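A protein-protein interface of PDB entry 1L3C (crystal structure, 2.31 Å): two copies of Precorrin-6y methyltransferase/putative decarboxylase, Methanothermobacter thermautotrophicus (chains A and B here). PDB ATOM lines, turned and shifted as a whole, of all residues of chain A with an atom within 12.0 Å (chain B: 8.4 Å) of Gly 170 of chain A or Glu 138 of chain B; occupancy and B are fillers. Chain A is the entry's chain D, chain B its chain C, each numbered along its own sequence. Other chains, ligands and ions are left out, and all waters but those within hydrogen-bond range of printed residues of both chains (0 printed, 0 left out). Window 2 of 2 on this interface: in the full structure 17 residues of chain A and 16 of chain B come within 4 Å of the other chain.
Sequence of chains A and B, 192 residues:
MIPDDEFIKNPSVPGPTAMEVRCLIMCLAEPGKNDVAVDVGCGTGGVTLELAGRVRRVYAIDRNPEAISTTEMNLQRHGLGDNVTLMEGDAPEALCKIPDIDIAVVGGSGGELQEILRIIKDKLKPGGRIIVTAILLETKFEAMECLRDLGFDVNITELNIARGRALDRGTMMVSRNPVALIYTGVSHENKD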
ATOM      1  N   ARG A 163       1.676  18.709  17.658  1.00  0.00           N
ATOM      2  CA  ARG A 163       0.243  18.862  17.688  1.00  0.00           C
ATOM      3  C   ARG A 163      -0.080  20.155  16.975  1.00  0.00           C
ATOM      4  O   ARG A 163       0.691  21.121  17.047  1.00  0.00           O
ATOM      5  CB  ARG A 163      -0.236  18.968  19.131  1.00  0.00           C
ATOM      6  CG  ARG A 163       0.095  17.773  19.984  1.00  0.00           C
ATOM      7  CD  ARG A 163      -0.466  17.974  21.352  1.00  0.00           C
ATOM      8  NE  ARG A 163      -0.071  16.914  22.269  1.00  0.00           N
ATOM      9  CZ  ARG A 163       0.132  17.098  23.575  1.00  0.00           C
ATOM     10  NH1 ARG A 163      -0.020  18.303  24.122  1.00  0.00           N
ATOM     11  NH2 ARG A 163       0.466  16.071  24.343  1.00  0.00           N
ATOM     12  N   GLY A 164      -1.230  20.200  16.319  1.00  0.00           N
ATOM     13  CA  GLY A 164      -1.597  21.411  15.618  1.00  0.00           C
ATOM     14  C   GLY A 164      -2.257  22.403  16.547  1.00  0.00           C
ATOM     15  O   GLY A 164      -3.015  22.014  17.444  1.00  0.00           O
ATOM     16  N   ARG A 165      -1.915  23.673  16.392  1.00  0.00           N
ATOM     17  CA  ARG A 165      -2.534  24.725  17.181  1.00  0.00           C
ATOM     18  C   ARG A 165      -3.272  25.641  16.203  1.00  0.00           C
ATOM     19  O   ARG A 165      -2.675  26.199  15.272  1.00  0.00           O
ATOM     20  CB  ARG A 165      -1.514  25.526  17.957  1.00  0.00           C
ATOM     21  CG  ARG A 165      -2.179  26.675  18.686  1.00  0.00           C
ATOM     22  CD  ARG A 165      -1.191  27.623  19.285  1.00  0.00           C
ATOM     23  NE  ARG A 165      -0.409  26.988  20.338  1.00  0.00           N
ATOM     24  CZ  ARG A 165       0.841  27.325  20.653  1.00  0.00           C
ATOM     25  NH1 ARG A 165       1.475  28.286  19.994  1.00  0.00           N
ATOM     26  NH2 ARG A 165       1.439  26.746  21.678  1.00  0.00           N
ATOM     27  N   ALA A 166      -4.584  25.746  16.390  1.00  0.00           N
ATOM     28  CA  ALA A 166      -5.413  26.558  15.521  1.00  0.00           C
ATOM     29  C   ALA A 166      -5.149  28.029  15.777  1.00  0.00           C
ATOM     30  O   ALA A 166      -5.248  28.500  16.907  1.00  0.00           O
ATOM     31  CB  ALA A 166      -6.890  26.221  15.728  1.00  0.00           C
ATOM     32  N   LEU A 167      -4.662  28.698  14.742  1.00  0.00           N
ATOM     33  CA  LEU A 167      -4.406  30.128  14.773  1.00  0.00           C
ATOM     34  C   LEU A 167      -5.366  30.677  13.727  1.00  0.00           C
ATOM     35  O   LEU A 167      -5.972  29.915  12.959  1.00  0.00           O
ATOM     36  CB  LEU A 167      -2.972  30.434  14.350  1.00  0.00           C
ATOM     37  CG  LEU A 167      -1.850  29.919  15.244  1.00  0.00           C
ATOM     38  CD1 LEU A 167      -0.532  30.292  14.633  1.00  0.00           C
ATOM     39  CD2 LEU A 167      -1.967  30.511  16.627  1.00  0.00           C
ATOM     40  N   ASP A 168      -5.474  31.992  13.648  1.00  0.00           N
ATOM     41  CA  ASP A 168      -6.380  32.584  12.675  1.00  0.00           C
ATOM     42  C   ASP A 168      -5.899  32.340  11.268  1.00  0.00           C
ATOM     43  O   ASP A 168      -6.676  32.001  10.378  1.00  0.00           O
ATOM     44  CB  ASP A 168      -6.525  34.080  12.911  1.00  0.00           C
ATOM     45  CG  ASP A 168      -7.975  34.520  12.918  1.00  0.00           C
ATOM     46  OD1 ASP A 168      -8.520  34.837  11.829  1.00  0.00           O
ATOM     47  OD2 ASP A 168      -8.575  34.527  14.021  1.00  0.00           O
ATOM     48  N   ARG A 169      -4.601  32.533  11.087  1.00  0.00           N
ATOM     49  CA  ARG A 169      -3.947  32.332   9.798  1.00  0.00           C
ATOM     50  C   ARG A 169      -3.898  30.858   9.355  1.00  0.00           C
ATOM     51  O   ARG A 169      -3.728  30.570   8.158  1.00  0.00           O
ATOM     52  CB  ARG A 169      -2.530  32.879   9.875  1.00  0.00           C
ATOM     53  CG  ARG A 169      -1.805  32.371  11.103  1.00  0.00           C
ATOM     54  CD  ARG A 169      -0.355  32.748  11.099  1.00  0.00           C
ATOM     55  NE  ARG A 169      -0.016  33.511  12.287  1.00  0.00           N
ATOM     56  CZ  ARG A 169       1.127  34.160  12.439  1.00  0.00           C
ATOM     57  NH1 ARG A 169       2.037  34.127  11.481  1.00  0.00           N
ATOM     58  NH2 ARG A 169       1.350  34.871  13.530  1.00  0.00           N
ATOM     59  N   GLY A 170      -3.976  29.942  10.326  1.00  0.00           N
ATOM     60  CA  GLY A 170      -3.950  28.524  10.022  1.00  0.00           C
ATOM     61  C   GLY A 170      -3.518  27.643  11.184  1.00  0.00           C
ATOM     62  O   GLY A 170      -3.515  28.050  12.334  1.00  0.00           O
ATOM     63  N   THR A 171      -3.154  26.409  10.868  1.00  0.00           N
ATOM     64  CA  THR A 171      -2.724  25.437  11.849  1.00  0.00           C
ATOM     65  C   THR A 171      -1.208  25.291  11.898  1.00  0.00           C
ATOM     66  O   THR A 171      -0.599  24.756  10.968  1.00  0.00           O
ATOM     67  CB  THR A 171      -3.296  24.076  11.502  1.00  0.00           C
ATOM     68  OG1 THR A 171      -4.694  24.207  11.276  1.00  0.00           O
ATOM     69  CG2 THR A 171      -3.085  23.119  12.618  1.00  0.00           C
ATOM     70  N   MET A 172      -0.582  25.773  12.963  1.00  0.00           N
ATOM     71  CA  MET A 172       0.855  25.613  13.062  1.00  0.00           C
ATOM     72  C   MET A 172       1.180  24.403  13.929  1.00  0.00           C
ATOM     73  O   MET A 172       0.479  24.100  14.878  1.00  0.00           O
ATOM     74  CB  MET A 172       1.526  26.859  13.600  1.00  0.00           C
ATOM     75  CG  MET A 172       1.470  27.004  15.072  1.00  0.00           C
ATOM     76  SD  MET A 172       2.957  28.137  15.736  1.00  0.00           S
ATOM     77  CE  MET A 172       1.931  29.139  17.053  1.00  0.00           C
ATOM     78  N   MET A 173       2.215  23.671  13.561  1.00  0.00           N
ATOM     79  CA  MET A 173       2.584  22.469  14.303  1.00  0.00           C
ATOM     80  C   MET A 173       3.512  22.851  15.436  1.00  0.00           C
ATOM     81  O   MET A 173       4.529  23.514  15.237  1.00  0.00           O
ATOM     82  CB  MET A 173       3.268  21.449  13.386  1.00  0.00           C
ATOM     83  CG  MET A 173       2.432  21.028  12.182  1.00  0.00           C
ATOM     84  SD  MET A 173       0.671  20.383  12.722  1.00  0.00           S
ATOM     85  CE  MET A 173       1.190  18.617  13.421  1.00  0.00           C
ATOM     86  N   VAL A 174       3.148  22.436  16.634  1.00  0.00           N
ATOM     87  CA  VAL A 174       3.930  22.752  17.809  1.00  0.00           C
ATOM     88  C   VAL A 174       4.502  21.481  18.396  1.00  0.00           C
ATOM     89  O   VAL A 174       3.787  20.537  18.700  1.00  0.00           O
ATOM     90  CB  VAL A 174       3.088  23.501  18.880  1.00  0.00           C
ATOM     91  CG1 VAL A 174       3.916  23.746  20.121  1.00  0.00           C
ATOM     92  CG2 VAL A 174       2.589  24.836  18.323  1.00  0.00           C
ATOM     93  N   SER B 109       4.531  34.012   4.780  1.00  0.00           N
ATOM     94  CA  SER B 109       3.626  34.081   3.636  1.00  0.00           C
ATOM     95  C   SER B 109       2.584  35.205   3.800  1.00  0.00           C
ATOM     96  O   SER B 109       2.085  35.756   2.810  1.00  0.00           O
ATOM     97  CB  SER B 109       2.937  32.726   3.468  1.00  0.00           C
ATOM     98  OG  SER B 109       2.441  32.260   4.718  1.00  0.00           O
ATOM     99  N   LEU B 113       0.305  34.124  -0.003  1.00  0.00           N
ATOM    100  CA  LEU B 113       1.296  33.237  -0.604  1.00  0.00           C
ATOM    101  C   LEU B 113       1.125  33.012  -2.085  1.00  0.00           C
ATOM    102  O   LEU B 113       2.069  33.173  -2.853  1.00  0.00           O
ATOM    103  CB  LEU B 113       1.327  31.893   0.117  1.00  0.00           C
ATOM    104  CG  LEU B 113       2.429  30.932  -0.328  1.00  0.00           C
ATOM    105  CD1 LEU B 113       3.793  31.556  -0.044  1.00  0.00           C
ATOM    106  CD2 LEU B 113       2.285  29.582   0.365  1.00  0.00           C
ATOM    107  N   ALA B 134       7.778  26.871   5.650  1.00  0.00           N
ATOM    108  CA  ALA B 134       6.440  26.593   6.167  1.00  0.00           C
ATOM    109  C   ALA B 134       6.380  26.125   7.626  1.00  0.00           C
ATOM    110  O   ALA B 134       7.085  25.217   8.039  1.00  0.00           O
ATOM    111  CB  ALA B 134       5.755  25.596   5.271  1.00  0.00           C
ATOM    112  N   ILE B 135       5.515  26.782   8.387  1.00  0.00           N
ATOM    113  CA  ILE B 135       5.276  26.504   9.791  1.00  0.00           C
ATOM    114  C   ILE B 135       3.867  25.961   9.905  1.00  0.00           C
ATOM    115  O   ILE B 135       3.574  25.133  10.774  1.00  0.00           O
ATOM    116  CB  ILE B 135       5.337  27.812  10.632  1.00  0.00           C
ATOM    117  CG1 ILE B 135       6.758  28.347  10.634  1.00  0.00           C
ATOM    118  CG2 ILE B 135       4.865  27.571  12.064  1.00  0.00           C
ATOM    119  CD1 ILE B 135       7.796  27.252  10.897  1.00  0.00           C
ATOM    120  N   LEU B 136       2.975  26.495   9.080  1.00  0.00           N
ATOM    121  CA  LEU B 136       1.603  26.061   9.100  1.00  0.00           C
ATOM    122  C   LEU B 136       1.428  24.901   8.166  1.00  0.00           C
ATOM    123  O   LEU B 136       2.107  24.792   7.156  1.00  0.00           O
ATOM    124  CB  LEU B 136       0.685  27.192   8.689  1.00  0.00           C
ATOM    125  CG  LEU B 136       0.940  28.470   9.478  1.00  0.00           C
ATOM    126  CD1 LEU B 136       0.066  29.552   8.940  1.00  0.00           C
ATOM    127  CD2 LEU B 136       0.661  28.262  10.925  1.00  0.00           C
ATOM    128  N   LEU B 137       0.527  24.013   8.542  1.00  0.00           N
ATOM    129  CA  LEU B 137       0.207  22.848   7.756  1.00  0.00           C
ATOM    130  C   LEU B 137      -0.363  23.273   6.392  1.00  0.00           C
ATOM    131  O   LEU B 137      -0.083  22.661   5.360  1.00  0.00           O
ATOM    132  CB  LEU B 137      -0.804  21.996   8.534  1.00  0.00           C
ATOM    133  CG  LEU B 137      -1.488  20.858   7.778  1.00  0.00           C
ATOM    134  CD1 LEU B 137      -0.439  19.843   7.310  1.00  0.00           C
ATOM    135  CD2 LEU B 137      -2.518  20.201   8.660  1.00  0.00           C
ATOM    136  N   GLU B 138      -1.126  24.355   6.385  1.00  0.00           N
ATOM    137  CA  GLU B 138      -1.756  24.854   5.155  1.00  0.00           C
ATOM    138  C   GLU B 138      -0.755  25.422   4.149  1.00  0.00           C
ATOM    139  O   GLU B 138      -0.914  25.261   2.936  1.00  0.00           O
ATOM    140  CB  GLU B 138      -2.842  25.876   5.485  1.00  0.00           C
ATOM    141  CG  GLU B 138      -3.993  25.303   6.323  1.00  0.00           C
ATOM    142  CD  GLU B 138      -3.692  25.282   7.825  1.00  0.00           C
ATOM    143  OE1 GLU B 138      -2.662  25.872   8.240  1.00  0.00           O
ATOM    144  OE2 GLU B 138      -4.491  24.675   8.580  1.00  0.00           O
ATOM    145  N   THR B 139       0.273  26.090   4.656  1.00  0.00           N
ATOM    146  CA  THR B 139       1.334  26.630   3.821  1.00  0.00           C
ATOM    147  C   THR B 139       2.089  25.484   3.132  1.00  0.00           C
ATOM    148  O   THR B 139       2.417  25.591   1.963  1.00  0.00           O
ATOM    149  CB  THR B 139       2.328  27.399   4.642  1.00  0.00           C
ATOM    150  OG1 THR B 139       1.646  28.400   5.393  1.00  0.00           O
ATOM    151  CG2 THR B 139       3.307  28.072   3.756  1.00  0.00           C
ATOM    152  N   LYS B 140       2.378  24.397   3.845  1.00  0.00           N
ATOM    153  CA  LYS B 140       3.073  23.267   3.241  1.00  0.00           C
ATOM    154  C   LYS B 140       2.300  22.783   2.037  1.00  0.00           C
ATOM    155  O   LYS B 140       2.870  22.545   0.990  1.00  0.00           O
ATOM    156  CB  LYS B 140       3.235  22.108   4.235  1.00  0.00           C
ATOM    157  CG  LYS B 140       3.961  22.512   5.493  1.00  0.00           C
ATOM    158  CD  LYS B 140       4.104  21.393   6.488  1.00  0.00           C
ATOM    159  CE  LYS B 140       4.755  21.943   7.764  1.00  0.00           C
ATOM    160  NZ  LYS B 140       4.693  20.994   8.923  1.00  0.00           N
ATOM    161  N   PHE B 141       0.990  22.670   2.186  1.00  0.00           N
ATOM    162  CA  PHE B 141       0.140  22.208   1.101  1.00  0.00           C
ATOM    163  C   PHE B 141       0.037  23.233  -0.031  1.00  0.00           C
ATOM    164  O   PHE B 141       0.311  22.923  -1.209  1.00  0.00           O
ATOM    165  CB  PHE B 141      -1.257  21.875   1.636  1.00  0.00           C
ATOM    166  CG  PHE B 141      -2.196  21.393   0.581  1.00  0.00           C
ATOM    167  CD1 PHE B 141      -2.094  20.088   0.091  1.00  0.00           C
ATOM    168  CD2 PHE B 141      -3.137  22.268   0.018  1.00  0.00           C
ATOM    169  CE1 PHE B 141      -2.906  19.668  -0.947  1.00  0.00           C
ATOM    170  CE2 PHE B 141      -3.952  21.858  -1.016  1.00  0.00           C
ATOM    171  CZ  PHE B 141      -3.837  20.557  -1.501  1.00  0.00           C
ATOM    172  N   GLU B 142      -0.379  24.444   0.333  1.00  0.00           N
ATOM    173  CA  GLU B 142      -0.560  25.543  -0.610  1.00  0.00           C
ATOM    174  C   GLU B 142       0.706  25.827  -1.457  1.00  0.00           C
ATOM    175  O   GLU B 142       0.606  25.952  -2.679  1.00  0.00           O
ATOM    176  CB  GLU B 142      -1.067  26.781   0.158  1.00  0.00           C
ATOM    177  CG  GLU B 142      -1.072  28.131  -0.611  1.00  0.00           C
ATOM    178  CD  GLU B 142      -2.339  28.413  -1.459  1.00  0.00           C
ATOM    179  OE1 GLU B 142      -2.983  27.442  -1.922  1.00  0.00           O
ATOM    180  OE2 GLU B 142      -2.674  29.614  -1.680  1.00  0.00           O
ATOM    181  N   ALA B 143       1.888  25.848  -0.827  1.00  0.00           N
ATOM    182  CA  ALA B 143       3.151  26.099  -1.526  1.00  0.00           C
ATOM    183  C   ALA B 143       3.412  25.020  -2.545  1.00  0.00           C
ATOM    184  O   ALA B 143       3.777  25.306  -3.672  1.00  0.00           O
ATOM    185  CB  ALA B 143       4.313  26.152  -0.564  1.00  0.00           C
ATOM    186  N   MET B 144       3.265  23.773  -2.131  1.00  0.00           N
ATOM    187  CA  MET B 144       3.466  22.635  -3.013  1.00  0.00           C
ATOM    188  C   MET B 144       2.579  22.750  -4.227  1.00  0.00           C
ATOM    189  O   MET B 144       3.032  22.591  -5.355  1.00  0.00           O
ATOM    190  CB  MET B 144       3.070  21.371  -2.284  1.00  0.00           C
ATOM    191  CG  MET B 144       4.057  20.932  -1.233  1.00  0.00           C
ATOM    192  SD  MET B 144       5.266  19.656  -2.025  1.00  0.00           S
ATOM    193  CE  MET B 144       3.872  18.385  -2.524  1.00  0.00           C
ATOM    194  N   GLU B 145       1.305  23.013  -3.972  1.00  0.00           N
ATOM    195  CA  GLU B 145       0.319  23.136  -5.018  1.00  0.00           C
ATOM    196  C   GLU B 145       0.593  24.302  -5.968  1.00  0.00           C
ATOM    197  O   GLU B 145       0.615  24.108  -7.183  1.00  0.00           O
ATOM    198  CB  GLU B 145      -1.065  23.260  -4.389  1.00  0.00           C
ATOM    199  CG  GLU B 145      -2.183  23.269  -5.392  1.00  0.00           C
ATOM    200  CD  GLU B 145      -3.528  23.508  -4.748  1.00  0.00           C
ATOM    201  OE1 GLU B 145      -3.673  24.471  -3.943  1.00  0.00           O
ATOM    202  OE2 GLU B 145      -4.441  22.716  -5.065  1.00  0.00           O
ATOM    203  N   ILE B 182       9.905  24.031   1.146  1.00  0.00           N
ATOM    204  CA  ILE B 182       9.364  23.653  -0.156  1.00  0.00           C
ATOM    205  C   ILE B 182      10.214  24.428  -1.145  1.00  0.00           C
ATOM    206  O   ILE B 182      10.328  25.649  -1.048  1.00  0.00           O
ATOM    207  CB  ILE B 182       7.880  24.013  -0.303  1.00  0.00           C
ATOM    208  CG1 ILE B 182       7.030  23.198   0.687  1.00  0.00           C
ATOM    209  CG2 ILE B 182       7.420  23.672  -1.700  1.00  0.00           C
ATOM    210  CD1 ILE B 182       6.843  23.847   2.048  1.00  0.00           C
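Of chain B, only Glu 138 comes within 4 Å of Gly 170 of chain A.
Glu 138 of chain B touches two residues of chain A.
Leu 137 of chain B touches just one residue of chain A: Thr 171 (2.8 Å).
Lys 140 of chain B touches one residue of chain A.
No residue of chain A comes within 4 Å of Phe 141 of chain B.
Glu 142 of chain B touches none of the printed residues of chain A.
Of the printed residues of chain B, Thr 171 of chain A touches Leu 136 (3.2 Å), Leu 137 (2.8 Å) and Glu 138 (2.7 Å).
Of the printed residues of chain B, Met 172 of chain A touches Ile 135 (3.6 Å) and Leu 136 (3.1 Å).
The nearest printed residue of chain B that does not touch Arg 169 of chain A is Glu 138 of chain B (4.8 Å).
O of Ile 135 of chain B lies within hydrogen-bond range of N of Met 173 of chain A, at 3.4 Å.
The backbone NH (N) of Leu 137 of chain B lies within hydrogen-bond range of the backbone carbonyl oxygen (O) of Thr 171 of chain A, at 2.8 Å.
The side-chain carboxylate (OE1) of Glu 138 of chain B lies within hydrogen-bond range of the backbone NH (N) of Thr 171 of chain A (2.7 Å).
Arg 169 of chain A touches Leu 136 of chain B.
OE1 of Glu 138 of chain B touches CA of Gly 170 of chain A, at 3.4 Å.
Thr 171 of chain A touches Leu 136 of chain B.
O of Ile 135 of chain B touches CA of Met 172 of chain A, at 3.6 Å.
Leu 136 of chain B touches Met 172 of chain A.
Lys 140 of chain B touches Met 173 of chain A (NZ to CG, 3.97 Å).
Of the 15 printed residues of chain B, 5 touch a printed residue of chain A.
Among the printed residues, no Asp or Glu carboxylate lies within 4 Å of a Lys or Arg side-chain nitrogen of the other chain.
No position is printed for both chains.
The backbone NH of Arg 165 of chain A lies within hydrogen-bond range of the backbone carbonyl oxygen of Met 172 of chain A, at 2.9 Å.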
